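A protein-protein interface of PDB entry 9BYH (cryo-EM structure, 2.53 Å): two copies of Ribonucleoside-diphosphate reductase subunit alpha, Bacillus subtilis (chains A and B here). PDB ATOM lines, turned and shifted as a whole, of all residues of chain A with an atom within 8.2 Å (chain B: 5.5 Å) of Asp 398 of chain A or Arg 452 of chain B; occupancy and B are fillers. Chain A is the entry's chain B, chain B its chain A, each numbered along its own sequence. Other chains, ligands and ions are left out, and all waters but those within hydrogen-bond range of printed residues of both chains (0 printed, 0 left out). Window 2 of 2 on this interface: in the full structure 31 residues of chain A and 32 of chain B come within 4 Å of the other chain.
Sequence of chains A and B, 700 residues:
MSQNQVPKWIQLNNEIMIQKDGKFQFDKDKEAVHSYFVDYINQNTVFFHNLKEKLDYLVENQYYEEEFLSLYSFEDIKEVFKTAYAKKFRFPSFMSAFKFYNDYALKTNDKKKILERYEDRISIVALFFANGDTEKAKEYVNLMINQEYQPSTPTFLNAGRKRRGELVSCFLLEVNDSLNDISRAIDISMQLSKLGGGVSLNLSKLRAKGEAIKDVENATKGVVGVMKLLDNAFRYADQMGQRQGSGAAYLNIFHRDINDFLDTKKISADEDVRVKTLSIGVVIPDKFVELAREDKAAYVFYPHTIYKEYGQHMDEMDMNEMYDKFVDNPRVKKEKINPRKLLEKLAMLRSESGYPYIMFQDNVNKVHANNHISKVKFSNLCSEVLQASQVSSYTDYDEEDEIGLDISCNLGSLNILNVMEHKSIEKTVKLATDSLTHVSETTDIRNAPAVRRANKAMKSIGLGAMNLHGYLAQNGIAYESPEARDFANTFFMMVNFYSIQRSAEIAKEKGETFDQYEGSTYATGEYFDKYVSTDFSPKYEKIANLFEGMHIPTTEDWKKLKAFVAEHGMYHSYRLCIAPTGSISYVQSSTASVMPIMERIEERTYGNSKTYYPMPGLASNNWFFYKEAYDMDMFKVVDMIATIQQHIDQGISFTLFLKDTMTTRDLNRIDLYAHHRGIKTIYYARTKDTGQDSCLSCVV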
ATOM      1  N   THR A 395      -6.068  -1.645  18.796  1.00  0.00           N
ATOM      2  CA  THR A 395      -7.482  -1.323  18.827  1.00  0.00           C
ATOM      3  C   THR A 395      -7.953  -1.151  20.270  1.00  0.00           C
ATOM      4  O   THR A 395      -7.156  -1.126  21.212  1.00  0.00           O
ATOM      5  CB  THR A 395      -8.275  -2.406  18.094  1.00  0.00           C
ATOM      6  OG1 THR A 395      -8.005  -3.681  18.689  1.00  0.00           O
ATOM      7  CG2 THR A 395      -7.880  -2.447  16.627  1.00  0.00           C
ATOM      8  N   ASP A 396      -9.264  -1.027  20.447  1.00  0.00           N
ATOM      9  CA  ASP A 396      -9.837  -0.873  21.773  1.00  0.00           C
ATOM     10  C   ASP A 396      -9.670  -2.155  22.583  1.00  0.00           C
ATOM     11  O   ASP A 396      -9.342  -3.219  22.055  1.00  0.00           O
ATOM     12  CB  ASP A 396     -11.320  -0.510  21.682  1.00  0.00           C
ATOM     13  CG  ASP A 396     -11.555   0.834  21.026  1.00  0.00           C
ATOM     14  OD1 ASP A 396     -10.628   1.670  21.026  1.00  0.00           O
ATOM     15  OD2 ASP A 396     -12.670   1.056  20.512  1.00  0.00           O
ATOM     16  N   TYR A 397      -9.892  -2.036  23.889  1.00  0.00           N
ATOM     17  CA  TYR A 397      -9.894  -3.210  24.747  1.00  0.00           C
ATOM     18  C   TYR A 397     -11.015  -4.155  24.332  1.00  0.00           C
ATOM     19  O   TYR A 397     -12.068  -3.729  23.850  1.00  0.00           O
ATOM     20  CB  TYR A 397     -10.055  -2.802  26.212  1.00  0.00           C
ATOM     21  CG  TYR A 397      -9.499  -3.810  27.190  1.00  0.00           C
ATOM     22  CD1 TYR A 397     -10.262  -4.889  27.614  1.00  0.00           C
ATOM     23  CD2 TYR A 397      -8.212  -3.681  27.693  1.00  0.00           C
ATOM     24  CE1 TYR A 397      -9.758  -5.812  28.507  1.00  0.00           C
ATOM     25  CE2 TYR A 397      -7.700  -4.598  28.587  1.00  0.00           C
ATOM     26  CZ  TYR A 397      -8.478  -5.660  28.991  1.00  0.00           C
ATOM     27  OH  TYR A 397      -7.973  -6.578  29.881  1.00  0.00           O
ATOM     28  N   ASP A 398     -10.765  -5.454  24.503  1.00  0.00           N
ATOM     29  CA  ASP A 398     -11.633  -6.545  24.070  1.00  0.00           C
ATOM     30  C   ASP A 398     -11.708  -6.661  22.553  1.00  0.00           C
ATOM     31  O   ASP A 398     -12.562  -7.392  22.035  1.00  0.00           O
ATOM     32  CB  ASP A 398     -13.051  -6.426  24.646  1.00  0.00           C
ATOM     33  CG  ASP A 398     -13.295  -7.381  25.797  1.00  0.00           C
ATOM     34  OD1 ASP A 398     -14.474  -7.612  26.139  1.00  0.00           O
ATOM     35  OD2 ASP A 398     -12.308  -7.899  26.361  1.00  0.00           O
ATOM     36  N   GLU A 399     -10.840  -5.962  21.827  1.00  0.00           N
ATOM     37  CA  GLU A 399     -10.739  -6.069  20.380  1.00  0.00           C
ATOM     38  C   GLU A 399      -9.335  -6.525  20.014  1.00  0.00           C
ATOM     39  O   GLU A 399      -8.355  -6.108  20.639  1.00  0.00           O
ATOM     40  CB  GLU A 399     -11.052  -4.733  19.697  1.00  0.00           C
ATOM     41  CG  GLU A 399     -12.475  -4.245  19.904  1.00  0.00           C
ATOM     42  CD  GLU A 399     -13.493  -5.083  19.155  1.00  0.00           C
ATOM     43  OE1 GLU A 399     -13.221  -5.454  17.993  1.00  0.00           O
ATOM     44  OE2 GLU A 399     -14.566  -5.370  19.727  1.00  0.00           O
ATOM     45  N   GLU A 400      -9.242  -7.387  19.005  1.00  0.00           N
ATOM     46  CA  GLU A 400      -7.947  -7.896  18.576  1.00  0.00           C
ATOM     47  C   GLU A 400      -7.132  -6.786  17.925  1.00  0.00           C
ATOM     48  O   GLU A 400      -7.653  -6.008  17.120  1.00  0.00           O
ATOM     49  CB  GLU A 400      -8.130  -9.060  17.604  1.00  0.00           C
ATOM     50  CG  GLU A 400      -8.360 -10.400  18.281  1.00  0.00           C
ATOM     51  CD  GLU A 400      -7.318 -10.706  19.337  1.00  0.00           C
ATOM     52  OE1 GLU A 400      -6.122 -10.785  18.989  1.00  0.00           O
ATOM     53  OE2 GLU A 400      -7.695 -10.867  20.517  1.00  0.00           O
ATOM     54  N   ASP A 401      -5.853  -6.715  18.277  1.00  0.00           N
ATOM     55  CA  ASP A 401      -4.947  -5.728  17.708  1.00  0.00           C
ATOM     56  C   ASP A 401      -4.240  -6.304  16.490  1.00  0.00           C
ATOM     57  O   ASP A 401      -3.859  -7.478  16.475  1.00  0.00           O
ATOM     58  CB  ASP A 401      -3.915  -5.278  18.743  1.00  0.00           C
ATOM     59  CG  ASP A 401      -4.550  -4.735  20.005  1.00  0.00           C
ATOM     60  OD1 ASP A 401      -5.734  -4.343  19.959  1.00  0.00           O
ATOM     61  OD2 ASP A 401      -3.863  -4.697  21.046  1.00  0.00           O
ATOM     62  N   ASP B 406     -13.873  -0.573  38.817  1.00  0.00           N
ATOM     63  CA  ASP B 406     -13.549   0.846  38.812  1.00  0.00           C
ATOM     64  C   ASP B 406     -14.842   1.646  38.836  1.00  0.00           C
ATOM     65  O   ASP B 406     -15.729   1.428  38.006  1.00  0.00           O
ATOM     66  CB  ASP B 406     -12.710   1.216  37.588  1.00  0.00           C
ATOM     67  CG  ASP B 406     -11.227   0.979  37.803  1.00  0.00           C
ATOM     68  OD1 ASP B 406     -10.851   0.462  38.875  1.00  0.00           O
ATOM     69  OD2 ASP B 406     -10.436   1.306  36.895  1.00  0.00           O
ATOM     70  N   ASP B 444     -21.643   2.091  27.797  1.00  0.00           N
ATOM     71  CA  ASP B 444     -20.762   0.991  27.404  1.00  0.00           C
ATOM     72  C   ASP B 444     -19.431   1.595  26.971  1.00  0.00           C
ATOM     73  O   ASP B 444     -19.318   2.141  25.869  1.00  0.00           O
ATOM     74  CB  ASP B 444     -21.383   0.155  26.291  1.00  0.00           C
ATOM     75  CG  ASP B 444     -21.315  -1.332  26.573  1.00  0.00           C
ATOM     76  OD1 ASP B 444     -20.948  -1.707  27.706  1.00  0.00           O
ATOM     77  OD2 ASP B 444     -21.629  -2.126  25.662  1.00  0.00           O
ATOM     78  N   ILE B 445     -18.428   1.495  27.837  1.00  0.00           N
ATOM     79  CA  ILE B 445     -17.100   2.038  27.576  1.00  0.00           C
ATOM     80  C   ILE B 445     -16.184   0.884  27.199  1.00  0.00           C
ATOM     81  O   ILE B 445     -15.954  -0.029  28.001  1.00  0.00           O
ATOM     82  CB  ILE B 445     -16.562   2.805  28.792  1.00  0.00           C
ATOM     83  CG1 ILE B 445     -17.474   3.993  29.103  1.00  0.00           C
ATOM     84  CG2 ILE B 445     -15.141   3.274  28.539  1.00  0.00           C
ATOM     85  CD1 ILE B 445     -17.137   4.699  30.385  1.00  0.00           C
ATOM     86  N   ARG B 446     -15.654   0.927  25.978  1.00  0.00           N
ATOM     87  CA  ARG B 446     -14.883  -0.173  25.420  1.00  0.00           C
ATOM     88  C   ARG B 446     -13.384  -0.035  25.651  1.00  0.00           C
ATOM     89  O   ARG B 446     -12.623  -0.903  25.213  1.00  0.00           O
ATOM     90  CB  ARG B 446     -15.161  -0.298  23.917  1.00  0.00           C
ATOM     91  CG  ARG B 446     -16.488   0.303  23.476  1.00  0.00           C
ATOM     92  CD  ARG B 446     -17.675  -0.511  23.977  1.00  0.00           C
ATOM     93  NE  ARG B 446     -17.925  -1.691  23.159  1.00  0.00           N
ATOM     94  CZ  ARG B 446     -18.515  -1.668  21.971  1.00  0.00           C
ATOM     95  NH1 ARG B 446     -18.926  -0.536  21.425  1.00  0.00           N
ATOM     96  NH2 ARG B 446     -18.698  -2.810  21.314  1.00  0.00           N
ATOM     97  N   ASN B 447     -12.941   1.025  26.326  1.00  0.00           N
ATOM     98  CA  ASN B 447     -11.528   1.231  26.608  1.00  0.00           C
ATOM     99  C   ASN B 447     -11.215   1.264  28.095  1.00  0.00           C
ATOM    100  O   ASN B 447     -10.046   1.433  28.464  1.00  0.00           O
ATOM    101  CB  ASN B 447     -11.041   2.530  25.950  1.00  0.00           C
ATOM    102  CG  ASN B 447     -10.536   2.312  24.541  1.00  0.00           C
ATOM    103  OD1 ASN B 447      -9.997   1.254  24.219  1.00  0.00           O
ATOM    104  ND2 ASN B 447     -10.717   3.311  23.688  1.00  0.00           N
ATOM    105  N   ALA B 448     -12.219   1.112  28.958  1.00  0.00           N
ATOM    106  CA  ALA B 448     -12.037   1.037  30.406  1.00  0.00           C
ATOM    107  C   ALA B 448     -12.681  -0.259  30.878  1.00  0.00           C
ATOM    108  O   ALA B 448     -13.888  -0.297  31.161  1.00  0.00           O
ATOM    109  CB  ALA B 448     -12.642   2.251  31.104  1.00  0.00           C
ATOM    110  N   PRO B 449     -11.915  -1.352  30.967  1.00  0.00           N
ATOM    111  CA  PRO B 449     -12.539  -2.646  31.287  1.00  0.00           C
ATOM    112  C   PRO B 449     -13.117  -2.703  32.688  1.00  0.00           C
ATOM    113  O   PRO B 449     -14.231  -3.207  32.873  1.00  0.00           O
ATOM    114  CB  PRO B 449     -11.388  -3.649  31.107  1.00  0.00           C
ATOM    115  CG  PRO B 449     -10.262  -2.881  30.479  1.00  0.00           C
ATOM    116  CD  PRO B 449     -10.455  -1.454  30.836  1.00  0.00           C
ATOM    117  N   ALA B 450     -12.389  -2.196  33.685  1.00  0.00           N
ATOM    118  CA  ALA B 450     -12.891  -2.232  35.053  1.00  0.00           C
ATOM    119  C   ALA B 450     -14.070  -1.287  35.245  1.00  0.00           C
ATOM    120  O   ALA B 450     -15.001  -1.611  35.988  1.00  0.00           O
ATOM    121  CB  ALA B 450     -11.768  -1.902  36.034  1.00  0.00           C
ATOM    122  N   VAL B 451     -14.057  -0.130  34.578  1.00  0.00           N
ATOM    123  CA  VAL B 451     -15.194   0.784  34.650  1.00  0.00           C
ATOM    124  C   VAL B 451     -16.443   0.119  34.085  1.00  0.00           C
ATOM    125  O   VAL B 451     -17.522   0.174  34.684  1.00  0.00           O
ATOM    126  CB  VAL B 451     -14.876   2.098  33.914  1.00  0.00           C
ATOM    127  CG1 VAL B 451     -16.151   2.870  33.618  1.00  0.00           C
ATOM    128  CG2 VAL B 451     -13.915   2.947  34.725  1.00  0.00           C
ATOM    129  N   ARG B 452     -16.310  -0.526  32.925  1.00  0.00           N
ATOM    130  CA  ARG B 452     -17.448  -1.206  32.314  1.00  0.00           C
ATOM    131  C   ARG B 452     -17.935  -2.362  33.179  1.00  0.00           C
ATOM    132  O   ARG B 452     -19.147  -2.550  33.356  1.00  0.00           O
ATOM    133  CB  ARG B 452     -17.065  -1.699  30.918  1.00  0.00           C
ATOM    134  CG  ARG B 452     -18.069  -2.642  30.285  1.00  0.00           C
ATOM    135  CD  ARG B 452     -17.647  -3.012  28.876  1.00  0.00           C
ATOM    136  NE  ARG B 452     -16.234  -3.368  28.813  1.00  0.00           N
ATOM    137  CZ  ARG B 452     -15.594  -3.707  27.702  1.00  0.00           C
ATOM    138  NH1 ARG B 452     -16.211  -3.743  26.532  1.00  0.00           N
ATOM    139  NH2 ARG B 452     -14.301  -4.016  27.767  1.00  0.00           N
ATOM    140  N   ARG B 453     -17.005  -3.146  33.731  1.00  0.00           N
ATOM    141  CA  ARG B 453     -17.393  -4.272  34.572  1.00  0.00           C
ATOM    142  C   ARG B 453     -18.117  -3.802  35.826  1.00  0.00           C
ATOM    143  O   ARG B 453     -19.132  -4.386  36.222  1.00  0.00           O
ATOM    144  CB  ARG B 453     -16.162  -5.103  34.936  1.00  0.00           C
ATOM    145  CG  ARG B 453     -16.366  -6.023  36.129  1.00  0.00           C
ATOM    146  CD  ARG B 453     -15.376  -7.172  36.126  1.00  0.00           C
ATOM    147  NE  ARG B 453     -14.614  -7.232  37.368  1.00  0.00           N
ATOM    148  CZ  ARG B 453     -15.021  -7.851  38.467  1.00  0.00           C
ATOM    149  NH1 ARG B 453     -16.182  -8.481  38.516  1.00  0.00           N
ATOM    150  NH2 ARG B 453     -14.242  -7.837  39.545  1.00  0.00           N
ATOM    151  N   ALA B 454     -17.619  -2.736  36.459  1.00  0.00           N
ATOM    152  CA  ALA B 454     -18.267  -2.221  37.657  1.00  0.00           C
ATOM    153  C   ALA B 454     -19.601  -1.563  37.339  1.00  0.00           C
ATOM    154  O   ALA B 454     -20.519  -1.609  38.161  1.00  0.00           O
ATOM    155  CB  ALA B 454     -17.345  -1.238  38.373  1.00  0.00           C
ATOM    156  N   ASN B 455     -19.733  -0.947  36.163  1.00  0.00           N
ATOM    157  CA  ASN B 455     -21.028  -0.407  35.767  1.00  0.00           C
ATOM    158  C   ASN B 455     -22.044  -1.523  35.558  1.00  0.00           C
ATOM    159  O   ASN B 455     -23.209  -1.389  35.946  1.00  0.00           O
ATOM    160  CB  ASN B 455     -20.882   0.436  34.501  1.00  0.00           C
ATOM    161  CG  ASN B 455     -22.190   1.066  34.068  1.00  0.00           C
ATOM    162  OD1 ASN B 455     -22.815   1.805  34.826  1.00  0.00           O
ATOM    163  ND2 ASN B 455     -22.612   0.775  32.844  1.00  0.00           N
ATOM    164  N   LYS B 456     -21.620  -2.628  34.944  1.00  0.00           N
ATOM    165  CA  LYS B 456     -22.531  -3.751  34.737  1.00  0.00           C
ATOM    166  C   LYS B 456     -22.889  -4.432  36.054  1.00  0.00           C
ATOM    167  O   LYS B 456     -24.034  -4.852  36.250  1.00  0.00           O
ATOM    168  CB  LYS B 456     -21.914  -4.756  33.766  1.00  0.00           C
ATOM    169  CG  LYS B 456     -22.469  -4.680  32.353  1.00  0.00           C
ATOM    170  CD  LYS B 456     -21.375  -4.842  31.300  1.00  0.00           C
ATOM    171  CE  LYS B 456     -20.240  -5.731  31.793  1.00  0.00           C
ATOM    172  NZ  LYS B 456     -19.122  -5.811  30.814  1.00  0.00           N
ATOM    173  N   ALA B 457     -21.924  -4.551  36.968  1.00  0.00           N
ATOM    174  CA  ALA B 457     -22.132  -5.325  38.187  1.00  0.00           C
ATOM    175  C   ALA B 457     -22.798  -4.497  39.281  1.00  0.00           C
ATOM    176  O   ALA B 457     -23.872  -4.849  39.777  1.00  0.00           O
ATOM    177  CB  ALA B 457     -20.795  -5.883  38.679  1.00  0.00           C
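The side-chain amide nitrogen of Asn 447 of chain B sits at hydrogen-bond distance from the side-chain carboxylate of Asp 396 of chain A (3.1 Å).
OD1 of Asn 447 of chain B lies within hydrogen-bond range of N of Tyr 397 of chain A (3.3 Å).
The side-chain carboxylate (OD1) of Asp 398 of chain A lies within salt-bridge range of the guanidinium group (NH2) of Arg 452 of chain B (3.95 Å).
The backbone NH (N) of Tyr 397 of chain A is in hydrogen-bond range of the backbone carbonyl oxygen (O) of Arg 446 of chain B.
The backbone carbonyl oxygen of Ile 445 of chain B sits at hydrogen-bond distance from the guanidinium group of Arg 452 of chain B (3.4 Å).
Of the printed residues of chain B, Asp 396 of chain A touches Arg 446 (3.8 Å) and Asn 447 (3.1 Å).
Of the printed residues of chain B, Tyr 397 of chain A touches Arg 446 (3.2 Å), Asn 447 (3.3 Å) and Pro 449 (3.5 Å).
Printed residues of chain B within 4 Å of Asp 398 of chain A: Arg 452.
Glu 399 of chain A touches none of the printed residues of chain B.
Printed residues of chain A within 4 Å of Arg 446 of chain B: Asp 396 (3.8 Å) and Tyr 397 (3.2 Å).
Printed residues of chain A within 4 Å of Asn 447 of chain B: Asp 396 (3.1 Å) and Tyr 397 (3.3 Å).
Of the printed residues of chain A, Pro 449 of chain B touches Tyr 397 (3.5 Å).
Of chain A, only Asp 398 comes within 4 Å of Arg 452 of chain B.
The nearest residue of chain B that does not touch Asp 398 of chain A is Arg 446 of chain B (5.0 Å).
The nearest residue of chain A that does not touch Arg 452 of chain B is Tyr 397 of chain A (4.1 Å).
The nearest printed residue of chain A that does not touch Pro 449 of chain B is Asp 398 of chain A (6.4 Å).
No position is printed for both chains.
Of the 6 pairs that touch across the chains among the printed residues, none has its exchanged pair printed and touching as well.
Of the 7 printed residues of chain A, 3 touch a printed residue of chain B.
Printed residues of chain A that touch a printed residue of chain B: Asp 396, Tyr 397 and Asp 398.
Hydrophobic or aromatic side chains of chain A that line the printed part of chain B: Tyr 397.
Of the 15 printed residues of chain B, 4 touch a printed residue of chain A.
Printed residues of chain B that touch a printed residue of chain A: Arg 446, Asn 447, Pro 449 and Arg 452.
Hydrophobic or aromatic side chains of chain B within 4 Å of the printed part of chain A: Pro 449.
Along chain B the printed residues that touch a printed residue of chain A span positions 446 to 452.
Among the printed residues, 6 pairs touch across the chains.
CB of Asp 396 of chain A touches O of Arg 446 of chain B, 3.8 Å away.
Pro 449 of chain B touches Tyr 397 of chain A (CG to CD1, 3.5 Å).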
